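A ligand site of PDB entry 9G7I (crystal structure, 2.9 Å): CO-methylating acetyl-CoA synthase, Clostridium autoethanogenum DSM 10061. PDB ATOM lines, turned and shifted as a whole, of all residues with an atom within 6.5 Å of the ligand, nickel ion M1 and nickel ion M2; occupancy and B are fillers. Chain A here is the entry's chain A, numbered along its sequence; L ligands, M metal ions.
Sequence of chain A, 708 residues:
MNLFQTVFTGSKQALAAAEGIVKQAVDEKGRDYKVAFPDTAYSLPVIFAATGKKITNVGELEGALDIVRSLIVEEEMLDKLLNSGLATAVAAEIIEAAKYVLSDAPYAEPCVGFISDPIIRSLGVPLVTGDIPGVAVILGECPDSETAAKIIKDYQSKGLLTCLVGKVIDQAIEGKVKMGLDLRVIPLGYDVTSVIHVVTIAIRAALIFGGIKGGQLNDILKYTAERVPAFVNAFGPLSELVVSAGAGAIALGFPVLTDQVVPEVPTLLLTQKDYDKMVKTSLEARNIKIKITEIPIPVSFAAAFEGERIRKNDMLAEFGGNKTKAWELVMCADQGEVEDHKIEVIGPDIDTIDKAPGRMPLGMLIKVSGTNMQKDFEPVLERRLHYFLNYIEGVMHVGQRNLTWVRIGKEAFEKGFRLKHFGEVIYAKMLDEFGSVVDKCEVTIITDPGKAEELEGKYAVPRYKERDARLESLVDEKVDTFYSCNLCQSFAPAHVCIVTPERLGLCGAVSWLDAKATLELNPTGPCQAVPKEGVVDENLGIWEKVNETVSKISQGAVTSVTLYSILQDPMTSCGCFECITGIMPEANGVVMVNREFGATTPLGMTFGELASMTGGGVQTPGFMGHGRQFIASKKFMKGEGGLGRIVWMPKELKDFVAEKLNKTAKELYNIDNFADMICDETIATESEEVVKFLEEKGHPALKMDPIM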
ATOM      1  N   ARG A 383      31.903   8.028   7.296  1.00  0.00           N
ATOM      2  CA  ARG A 383      30.453   8.353   7.366  1.00  0.00           C
ATOM      3  C   ARG A 383      30.168   9.059   8.698  1.00  0.00           C
ATOM      4  O   ARG A 383      29.490  10.097   8.676  1.00  0.00           O
ATOM      5  CB  ARG A 383      29.611   7.083   7.239  1.00  0.00           C
ATOM      6  CG  ARG A 383      28.115   7.304   7.440  1.00  0.00           C
ATOM      7  CD  ARG A 383      27.519   8.189   6.358  1.00  0.00           C
ATOM      8  NE  ARG A 383      26.138   8.544   6.645  1.00  0.00           N
ATOM      9  CZ  ARG A 383      25.557   9.665   6.222  1.00  0.00           C
ATOM     10  NH1 ARG A 383      26.246  10.549   5.518  1.00  0.00           N
ATOM     11  NH2 ARG A 383      24.286   9.896   6.517  1.00  0.00           N
ATOM     12  N   TYR A 387      28.145  13.042  10.836  1.00  0.00           N
ATOM     13  CA  TYR A 387      27.306  13.203  12.026  1.00  0.00           C
ATOM     14  C   TYR A 387      27.996  14.059  13.087  1.00  0.00           C
ATOM     15  O   TYR A 387      27.366  14.959  13.636  1.00  0.00           O
ATOM     16  CB  TYR A 387      26.915  11.824  12.594  1.00  0.00           C
ATOM     17  CG  TYR A 387      26.045  11.025  11.646  1.00  0.00           C
ATOM     18  CD1 TYR A 387      26.611  10.267  10.632  1.00  0.00           C
ATOM     19  CD2 TYR A 387      24.661  11.042  11.754  1.00  0.00           C
ATOM     20  CE1 TYR A 387      25.822   9.544   9.752  1.00  0.00           C
ATOM     21  CE2 TYR A 387      23.859  10.312  10.872  1.00  0.00           C
ATOM     22  CZ  TYR A 387      24.447   9.575   9.864  1.00  0.00           C
ATOM     23  OH  TYR A 387      23.675   8.849   8.983  1.00  0.00           O
ATOM     24  N   CYS A 485      19.686  -0.280   6.786  1.00  0.00           N
ATOM     25  CA  CYS A 485      20.125   0.793   7.674  1.00  0.00           C
ATOM     26  C   CYS A 485      18.940   1.659   8.087  1.00  0.00           C
ATOM     27  O   CYS A 485      18.064   1.929   7.257  1.00  0.00           O
ATOM     28  CB  CYS A 485      21.215   1.630   7.009  1.00  0.00           C
ATOM     29  SG  CYS A 485      21.732   3.071   7.994  1.00  0.00           S
ATOM     30  N   ASN A 486      18.913   2.097   9.351  1.00  0.00           N
ATOM     31  CA  ASN A 486      17.844   2.935   9.879  1.00  0.00           C
ATOM     32  C   ASN A 486      18.412   4.161  10.612  1.00  0.00           C
ATOM     33  O   ASN A 486      17.777   4.686  11.521  1.00  0.00           O
ATOM     34  CB  ASN A 486      16.958   2.124  10.829  1.00  0.00           C
ATOM     35  CG  ASN A 486      17.683   1.617  12.055  1.00  0.00           C
ATOM     36  OD1 ASN A 486      18.420   0.626  11.994  1.00  0.00           O
ATOM     37  ND2 ASN A 486      17.492   2.275  13.189  1.00  0.00           N
ATOM     38  N   LEU A 487      19.611   4.623  10.207  1.00  0.00           N
ATOM     39  CA  LEU A 487      20.247   5.785  10.820  1.00  0.00           C
ATOM     40  C   LEU A 487      19.518   7.069  10.419  1.00  0.00           C
ATOM     41  O   LEU A 487      19.381   7.981  11.240  1.00  0.00           O
ATOM     42  CB  LEU A 487      21.742   5.842  10.420  1.00  0.00           C
ATOM     43  CG  LEU A 487      22.736   6.426  11.427  1.00  0.00           C
ATOM     44  CD1 LEU A 487      22.537   5.869  12.843  1.00  0.00           C
ATOM     45  CD2 LEU A 487      24.177   6.177  10.957  1.00  0.00           C
ATOM     46  N   CYS A 488      18.960   7.104   9.210  1.00  0.00           N
ATOM     47  CA  CYS A 488      18.217   8.301   8.736  1.00  0.00           C
ATOM     48  C   CYS A 488      16.826   8.362   9.380  1.00  0.00           C
ATOM     49  O   CYS A 488      16.090   9.326   9.082  1.00  0.00           O
ATOM     50  CB  CYS A 488      18.052   8.261   7.229  1.00  0.00           C
ATOM     51  SG  CYS A 488      19.573   8.713   6.342  1.00  0.00           S
ATOM     52  N   GLN A 489      16.490   7.386  10.221  1.00  0.00           N
ATOM     53  CA  GLN A 489      15.163   7.350  10.831  1.00  0.00           C
ATOM     54  C   GLN A 489      14.973   8.472  11.881  1.00  0.00           C
ATOM     55  O   GLN A 489      13.875   8.646  12.389  1.00  0.00           O
ATOM     56  CB  GLN A 489      14.900   5.968  11.461  1.00  0.00           C
ATOM     57  CG  GLN A 489      13.419   5.583  11.505  1.00  0.00           C
ATOM     58  CD  GLN A 489      13.195   4.160  11.970  1.00  0.00           C
ATOM     59  OE1 GLN A 489      14.105   3.336  11.982  1.00  0.00           O
ATOM     60  NE2 GLN A 489      11.972   3.853  12.368  1.00  0.00           N
ATOM     61  N   PHE A 491      15.104  11.698  11.286  1.00  0.00           N
ATOM     62  CA  PHE A 491      14.246  12.699  10.639  1.00  0.00           C
ATOM     63  C   PHE A 491      13.115  12.028   9.854  1.00  0.00           C
ATOM     64  O   PHE A 491      11.974  12.499   9.918  1.00  0.00           O
ATOM     65  CB  PHE A 491      15.068  13.638   9.733  1.00  0.00           C
ATOM     66  CG  PHE A 491      16.018  12.989   8.758  1.00  0.00           C
ATOM     67  CD1 PHE A 491      17.254  12.542   9.168  1.00  0.00           C
ATOM     68  CD2 PHE A 491      15.702  12.911   7.415  1.00  0.00           C
ATOM     69  CE1 PHE A 491      18.148  11.982   8.262  1.00  0.00           C
ATOM     70  CE2 PHE A 491      16.589  12.345   6.514  1.00  0.00           C
ATOM     71  CZ  PHE A 491      17.809  11.896   6.939  1.00  0.00           C
ATOM     72  N   HIS A 495      11.759   5.558   7.119  1.00  0.00           N
ATOM     73  CA  HIS A 495      12.803   5.253   6.136  1.00  0.00           C
ATOM     74  C   HIS A 495      13.637   4.061   6.557  1.00  0.00           C
ATOM     75  O   HIS A 495      14.243   4.072   7.638  1.00  0.00           O
ATOM     76  CB  HIS A 495      13.713   6.467   5.915  1.00  0.00           C
ATOM     77  CG  HIS A 495      14.805   6.211   4.925  1.00  0.00           C
ATOM     78  ND1 HIS A 495      14.578   6.300   3.567  1.00  0.00           N
ATOM     79  CD2 HIS A 495      16.097   5.851   5.131  1.00  0.00           C
ATOM     80  CE1 HIS A 495      15.735   6.015   2.990  1.00  0.00           C
ATOM     81  NE2 HIS A 495      16.673   5.729   3.888  1.00  0.00           N
ATOM     82  N   VAL A 496      13.688   3.036   5.701  1.00  0.00           N
ATOM     83  CA  VAL A 496      14.480   1.835   5.918  1.00  0.00           C
ATOM     84  C   VAL A 496      15.311   1.660   4.657  1.00  0.00           C
ATOM     85  O   VAL A 496      14.791   1.145   3.667  1.00  0.00           O
ATOM     86  CB  VAL A 496      13.609   0.576   6.190  1.00  0.00           C
ATOM     87  CG1 VAL A 496      14.451  -0.552   6.811  1.00  0.00           C
ATOM     88  CG2 VAL A 496      12.406   0.896   7.071  1.00  0.00           C
ATOM     89  N   CYS A 497      16.578   2.058   4.706  1.00  0.00           N
ATOM     90  CA  CYS A 497      17.408   2.012   3.473  1.00  0.00           C
ATOM     91  C   CYS A 497      18.011   0.629   3.233  1.00  0.00           C
ATOM     92  O   CYS A 497      18.929   0.256   3.983  1.00  0.00           O
ATOM     93  CB  CYS A 497      18.536   3.052   3.530  1.00  0.00           C
ATOM     94  SG  CYS A 497      19.259   3.458   1.922  1.00  0.00           S
ATOM     95  N   ILE A 498      17.498  -0.101   2.231  1.00  0.00           N
ATOM     96  CA  ILE A 498      18.108  -1.416   1.873  1.00  0.00           C
ATOM     97  C   ILE A 498      19.376  -1.099   1.075  1.00  0.00           C
ATOM     98  O   ILE A 498      19.401  -0.052   0.393  1.00  0.00           O
ATOM     99  CB  ILE A 498      17.116  -2.283   1.078  1.00  0.00           C
ATOM    100  CG1 ILE A 498      15.824  -2.521   1.851  1.00  0.00           C
ATOM    101  CG2 ILE A 498      17.769  -3.588   0.654  1.00  0.00           C
ATOM    102  CD1 ILE A 498      16.031  -3.115   3.220  1.00  0.00           C
ATOM    103  N   VAL A 499      20.402  -1.942   1.173  1.00  0.00           N
ATOM    104  CA  VAL A 499      21.696  -1.631   0.499  1.00  0.00           C
ATOM    105  C   VAL A 499      22.179  -2.870  -0.263  1.00  0.00           C
ATOM    106  O   VAL A 499      22.157  -3.965   0.328  1.00  0.00           O
ATOM    107  CB  VAL A 499      22.737  -1.173   1.529  1.00  0.00           C
ATOM    108  CG1 VAL A 499      24.053  -0.779   0.882  1.00  0.00           C
ATOM    109  CG2 VAL A 499      22.212  -0.042   2.405  1.00  0.00           C
ATOM    110  N   LEU A 504      23.033   1.573  -3.852  1.00  0.00           N
ATOM    111  CA  LEU A 504      23.842   2.006  -2.681  1.00  0.00           C
ATOM    112  C   LEU A 504      22.982   2.817  -1.707  1.00  0.00           C
ATOM    113  O   LEU A 504      21.886   3.262  -2.108  1.00  0.00           O
ATOM    114  CB  LEU A 504      25.002   2.842  -3.207  1.00  0.00           C
ATOM    115  CG  LEU A 504      26.099   2.030  -3.868  1.00  0.00           C
ATOM    116  CD1 LEU A 504      26.903   2.859  -4.854  1.00  0.00           C
ATOM    117  CD2 LEU A 504      27.015   1.440  -2.802  1.00  0.00           C
ATOM    118  N   GLY A 505      23.469   2.996  -0.470  1.00  0.00           N
ATOM    119  CA  GLY A 505      22.748   3.844   0.497  1.00  0.00           C
ATOM    120  C   GLY A 505      22.477   5.205  -0.101  1.00  0.00           C
ATOM    121  O   GLY A 505      23.437   5.812  -0.629  1.00  0.00           O
ATOM    122  N   LEU A 506      21.241   5.665  -0.044  1.00  0.00           N
ATOM    123  CA  LEU A 506      20.872   6.939  -0.668  1.00  0.00           C
ATOM    124  C   LEU A 506      21.856   8.053  -0.291  1.00  0.00           C
ATOM    125  O   LEU A 506      22.000   9.027  -1.030  1.00  0.00           O
ATOM    126  CB  LEU A 506      19.437   7.360  -0.313  1.00  0.00           C
ATOM    127  CG  LEU A 506      18.327   6.305  -0.466  1.00  0.00           C
ATOM    128  CD1 LEU A 506      16.962   6.931  -0.298  1.00  0.00           C
ATOM    129  CD2 LEU A 506      18.398   5.589  -1.809  1.00  0.00           C
ATOM    130  N   CYS A 507      22.551   7.929   0.832  1.00  0.00           N
ATOM    131  CA  CYS A 507      23.449   9.065   1.190  1.00  0.00           C
ATOM    132  C   CYS A 507      24.688   9.060   0.300  1.00  0.00           C
ATOM    133  O   CYS A 507      25.325  10.127   0.173  1.00  0.00           O
ATOM    134  CB  CYS A 507      23.864   9.002   2.647  1.00  0.00           C
ATOM    135  SG  CYS A 507      24.823   7.517   3.011  1.00  0.00           S
ATOM    136  N   GLY A 508      24.998   7.924  -0.333  1.00  0.00           N
ATOM    137  CA  GLY A 508      26.133   7.835  -1.269  1.00  0.00           C
ATOM    138  C   GLY A 508      27.390   7.305  -0.589  1.00  0.00           C
ATOM    139  O   GLY A 508      28.345   6.967  -1.304  1.00  0.00           O
ATOM    140  N   ALA A 509      27.375   7.222   0.741  1.00  0.00           N
ATOM    141  CA  ALA A 509      28.575   6.780   1.489  1.00  0.00           C
ATOM    142  C   ALA A 509      28.480   5.285   1.808  1.00  0.00           C
ATOM    143  O   ALA A 509      29.307   4.515   1.273  1.00  0.00           O
ATOM    144  CB  ALA A 509      28.725   7.601   2.749  1.00  0.00           C
ATOM    145  N   VAL A 510      27.515   4.897   2.640  1.00  0.00           N
ATOM    146  CA  VAL A 510      27.405   3.473   3.072  1.00  0.00           C
ATOM    147  C   VAL A 510      27.263   2.576   1.839  1.00  0.00           C
ATOM    148  O   VAL A 510      26.290   2.746   1.091  1.00  0.00           O
ATOM    149  CB  VAL A 510      26.221   3.269   4.039  1.00  0.00           C
ATOM    150  CG1 VAL A 510      26.046   1.797   4.413  1.00  0.00           C
ATOM    151  CG2 VAL A 510      26.364   4.125   5.288  1.00  0.00           C
ATOM    152  N   SER A 511      28.216   1.649   1.636  1.00  0.00           N
ATOM    153  CA  SER A 511      28.144   0.693   0.508  1.00  0.00           C
ATOM    154  C   SER A 511      27.787  -0.691   1.073  1.00  0.00           C
ATOM    155  O   SER A 511      27.926  -0.861   2.302  1.00  0.00           O
ATOM    156  CB  SER A 511      29.430   0.656  -0.259  1.00  0.00           C
ATOM    157  OG  SER A 511      30.320  -0.292   0.316  1.00  0.00           O
ATOM    158  N   PRO A 526      22.796   0.283  13.237  1.00  0.00           N
ATOM    159  CA  PRO A 526      21.751   0.508  12.226  1.00  0.00           C
ATOM    160  C   PRO A 526      21.791  -0.517  11.086  1.00  0.00           C
ATOM    161  O   PRO A 526      20.742  -1.004  10.666  1.00  0.00           O
ATOM    162  CB  PRO A 526      22.043   1.930  11.728  1.00  0.00           C
ATOM    163  CG  PRO A 526      23.501   2.109  11.937  1.00  0.00           C
ATOM    164  CD  PRO A 526      23.882   1.287  13.135  1.00  0.00           C
ATOM    165  N   CYS A 527      22.989  -0.847  10.597  1.00  0.00           N
ATOM    166  CA  CYS A 527      23.155  -1.805   9.514  1.00  0.00           C
ATOM    167  C   CYS A 527      22.970  -3.228  10.038  1.00  0.00           C
ATOM    168  O   CYS A 527      23.848  -3.750  10.717  1.00  0.00           O
ATOM    169  CB  CYS A 527      24.515  -1.640   8.849  1.00  0.00           C
ATOM    170  SG  CYS A 527      24.790   0.010   8.143  1.00  0.00           S
ATOM    171  N   SER A 573      12.593   7.458   0.398  1.00  0.00           N
ATOM    172  CA  SER A 573      13.743   8.361   0.342  1.00  0.00           C
ATOM    173  C   SER A 573      13.852   9.150   1.667  1.00  0.00           C
ATOM    174  O   SER A 573      12.843   9.361   2.334  1.00  0.00           O
ATOM    175  CB  SER A 573      13.634   9.307  -0.854  1.00  0.00           C
ATOM    176  OG  SER A 573      13.491   8.577  -2.061  1.00  0.00           O
ATOM    177  N   CYS A 574      15.068   9.569   2.052  1.00  0.00           N
ATOM    178  CA  CYS A 574      15.294  10.277   3.309  1.00  0.00           C
ATOM    179  C   CYS A 574      15.512  11.803   3.146  1.00  0.00           C
ATOM    180  O   CYS A 574      14.561  12.568   3.310  1.00  0.00           O
ATOM    181  CB  CYS A 574      16.446   9.627   4.079  1.00  0.00           C
ATOM    182  SG  CYS A 574      17.851   9.145   3.049  1.00  0.00           S
ATOM    183  N   GLY A 575      16.738  12.236   2.828  1.00  0.00           N
ATOM    184  CA  GLY A 575      17.032  13.649   2.662  1.00  0.00           C
ATOM    185  C   GLY A 575      18.491  13.977   2.377  1.00  0.00           C
ATOM    186  O   GLY A 575      18.848  15.149   2.219  1.00  0.00           O
ATOM    187  N   CYS A 576      19.352  12.955   2.316  1.00  0.00           N
ATOM    188  CA  CYS A 576      20.790  13.101   2.053  1.00  0.00           C
ATOM    189  C   CYS A 576      21.169  12.760   0.616  1.00  0.00           C
ATOM    190  O   CYS A 576      22.359  12.690   0.310  1.00  0.00           O
ATOM    191  CB  CYS A 576      21.568  12.236   3.038  1.00  0.00           C
ATOM    192  SG  CYS A 576      21.027  10.508   3.077  1.00  0.00           S
ATOM    193  N   PHE A 577      20.165  12.602  -0.248  1.00  0.00           N
ATOM    194  CA  PHE A 577      20.409  12.247  -1.671  1.00  0.00           C
ATOM    195  C   PHE A 577      21.144  13.388  -2.373  1.00  0.00           C
ATOM    196  O   PHE A 577      20.714  14.547  -2.250  1.00  0.00           O
ATOM    197  CB  PHE A 577      19.091  11.911  -2.376  1.00  0.00           C
ATOM    198  CG  PHE A 577      17.848  12.659  -1.941  1.00  0.00           C
ATOM    199  CD1 PHE A 577      17.650  13.983  -2.292  1.00  0.00           C
ATOM    200  CD2 PHE A 577      16.853  12.025  -1.219  1.00  0.00           C
ATOM    201  CE1 PHE A 577      16.509  14.660  -1.913  1.00  0.00           C
ATOM    202  CE2 PHE A 577      15.705  12.697  -0.834  1.00  0.00           C
ATOM    203  CZ  PHE A 577      15.525  14.018  -1.187  1.00  0.00           C
HETATM  204 FE1  LIG L   1      22.061   4.623   5.995  1.00  0.00          FE
HETATM  205 FE2  LIG L   1      20.785   4.918   3.739  1.00  0.00          FE
HETATM  206 FE3  LIG L   1      23.064   6.207   4.135  1.00  0.00          FE
HETATM  207 FE4  LIG L   1      20.877   6.893   5.474  1.00  0.00          FE
HETATM  208  S1  LIG L   1      21.171   7.114   3.205  1.00  0.00           S
HETATM  209  S2  LIG L   1      22.975   6.705   6.383  1.00  0.00           S
HETATM  210  S3  LIG L   1      19.792   4.905   5.815  1.00  0.00           S
HETATM  211  S4  LIG L   1      22.847   3.939   3.940  1.00  0.00           S
HETATM  212 NI    NI M   1      19.614   9.416   4.077  1.00  0.00          NI
HETATM  213 NI    NI M   2      18.480  11.291   2.640  1.00  0.00          NI
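A ring nitrogen (NE2) of His 495 lies close to a sulfur (S3) of the ligand (3.8 Å).
An iron atom (FE1) of the ligand is bound by the side-chain sulfur (SG) of Cys 485.
NH2 of Arg 383 lies close to S2 of the ligand (3.5 Å).
S2 of the ligand lies close to OH of Tyr 387, at 3.4 Å.
SG of Cys 497 binds FE2 of the ligand (2.8 Å).
An iron atom (FE4) of the ligand is bound by the side-chain sulfur (SG) of Cys 488 (2.4 Å).
An iron atom (FE3) of the ligand is bound by the side-chain sulfur (SG) of Cys 507 (2.5 Å).
The backbone NH of Cys 507 lies close to a sulfur (S1) of the ligand, at 2.9 Å.
A sulfur (S1) of the ligand lies close to the backbone NH (N) of Leu 506 (3.6 Å).
O of Val 510 sits at hydrogen-bond distance from N of Gly 505 (3.2 Å).
The side-chain sulfur (SG) of Cys 485 sits close to the backbone NH (N) of Leu 487, 3.4 Å away.
The backbone NH (N) of Cys 485 lies within hydrogen-bond range of the backbone carbonyl oxygen (O) of Cys 497 (3.0 Å).
The side-chain sulfur of Cys 576 lies close to the backbone NH of Cys 507 (3.7 Å).
The side-chain sulfur (SG) of Cys 574 sits close to a ring nitrogen (NE2) of His 495 (3.7 Å).
N of Ala 509 sits close to SG of Cys 507 (3.4 Å).
N of Leu 506 sits close to SG of Cys 497 (3.6 Å).
OH of Tyr 387 is in hydrogen-bond range of NH2 of Arg 383.
Gly 505 touches the ligand.
Val 510 touches the ligand (CB to S4, 3.4 Å).
Hydrophobic or aromatic side chains that line the ligand: His 495, Leu 506 and Val 510.
12 residues have an atom within 4 Å of the ligand: Arg 383, Tyr 387, Cys 485, Cys 488, His 495, Cys 497, Gly 505, Leu 506, Cys 507, Val 510, Cys 574 and Cys 576.
The nearest printed residue that does not touch the ligand is Leu 487 (4.3 Å).
The nearest printed residue that does not touch nickel ion M1 is Phe 491 (4.2 Å).
Phe 577 touches nickel ion M2.
Within 4 Å of nickel ion M2: Cys 574, Gly 575, Cys 576 and Phe 577.
Along chain A the residues within 4 Å of nickel ion M2 span positions 574 to 577.
Nickel ion M1 is bound by SG of Cys 576 (2.0 Å), SG of Cys 574 (2.1 Å) and SG of Cys 488 (2.4 Å).
Nickel ion M1 has three donor atoms within binding distance.
Slightly farther from nickel ion M1 lies a sulfur (S1) of the ligand (2.9 Å).
Nickel ion M2 is bound by N of Cys 576 (1.9 Å), N of Gly 575 (2.0 Å), SG of Cys 574 (2.3 Å) and SG of Cys 576 (2.7 Å).
Nickel ion M2 has four donor atoms within binding distance.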
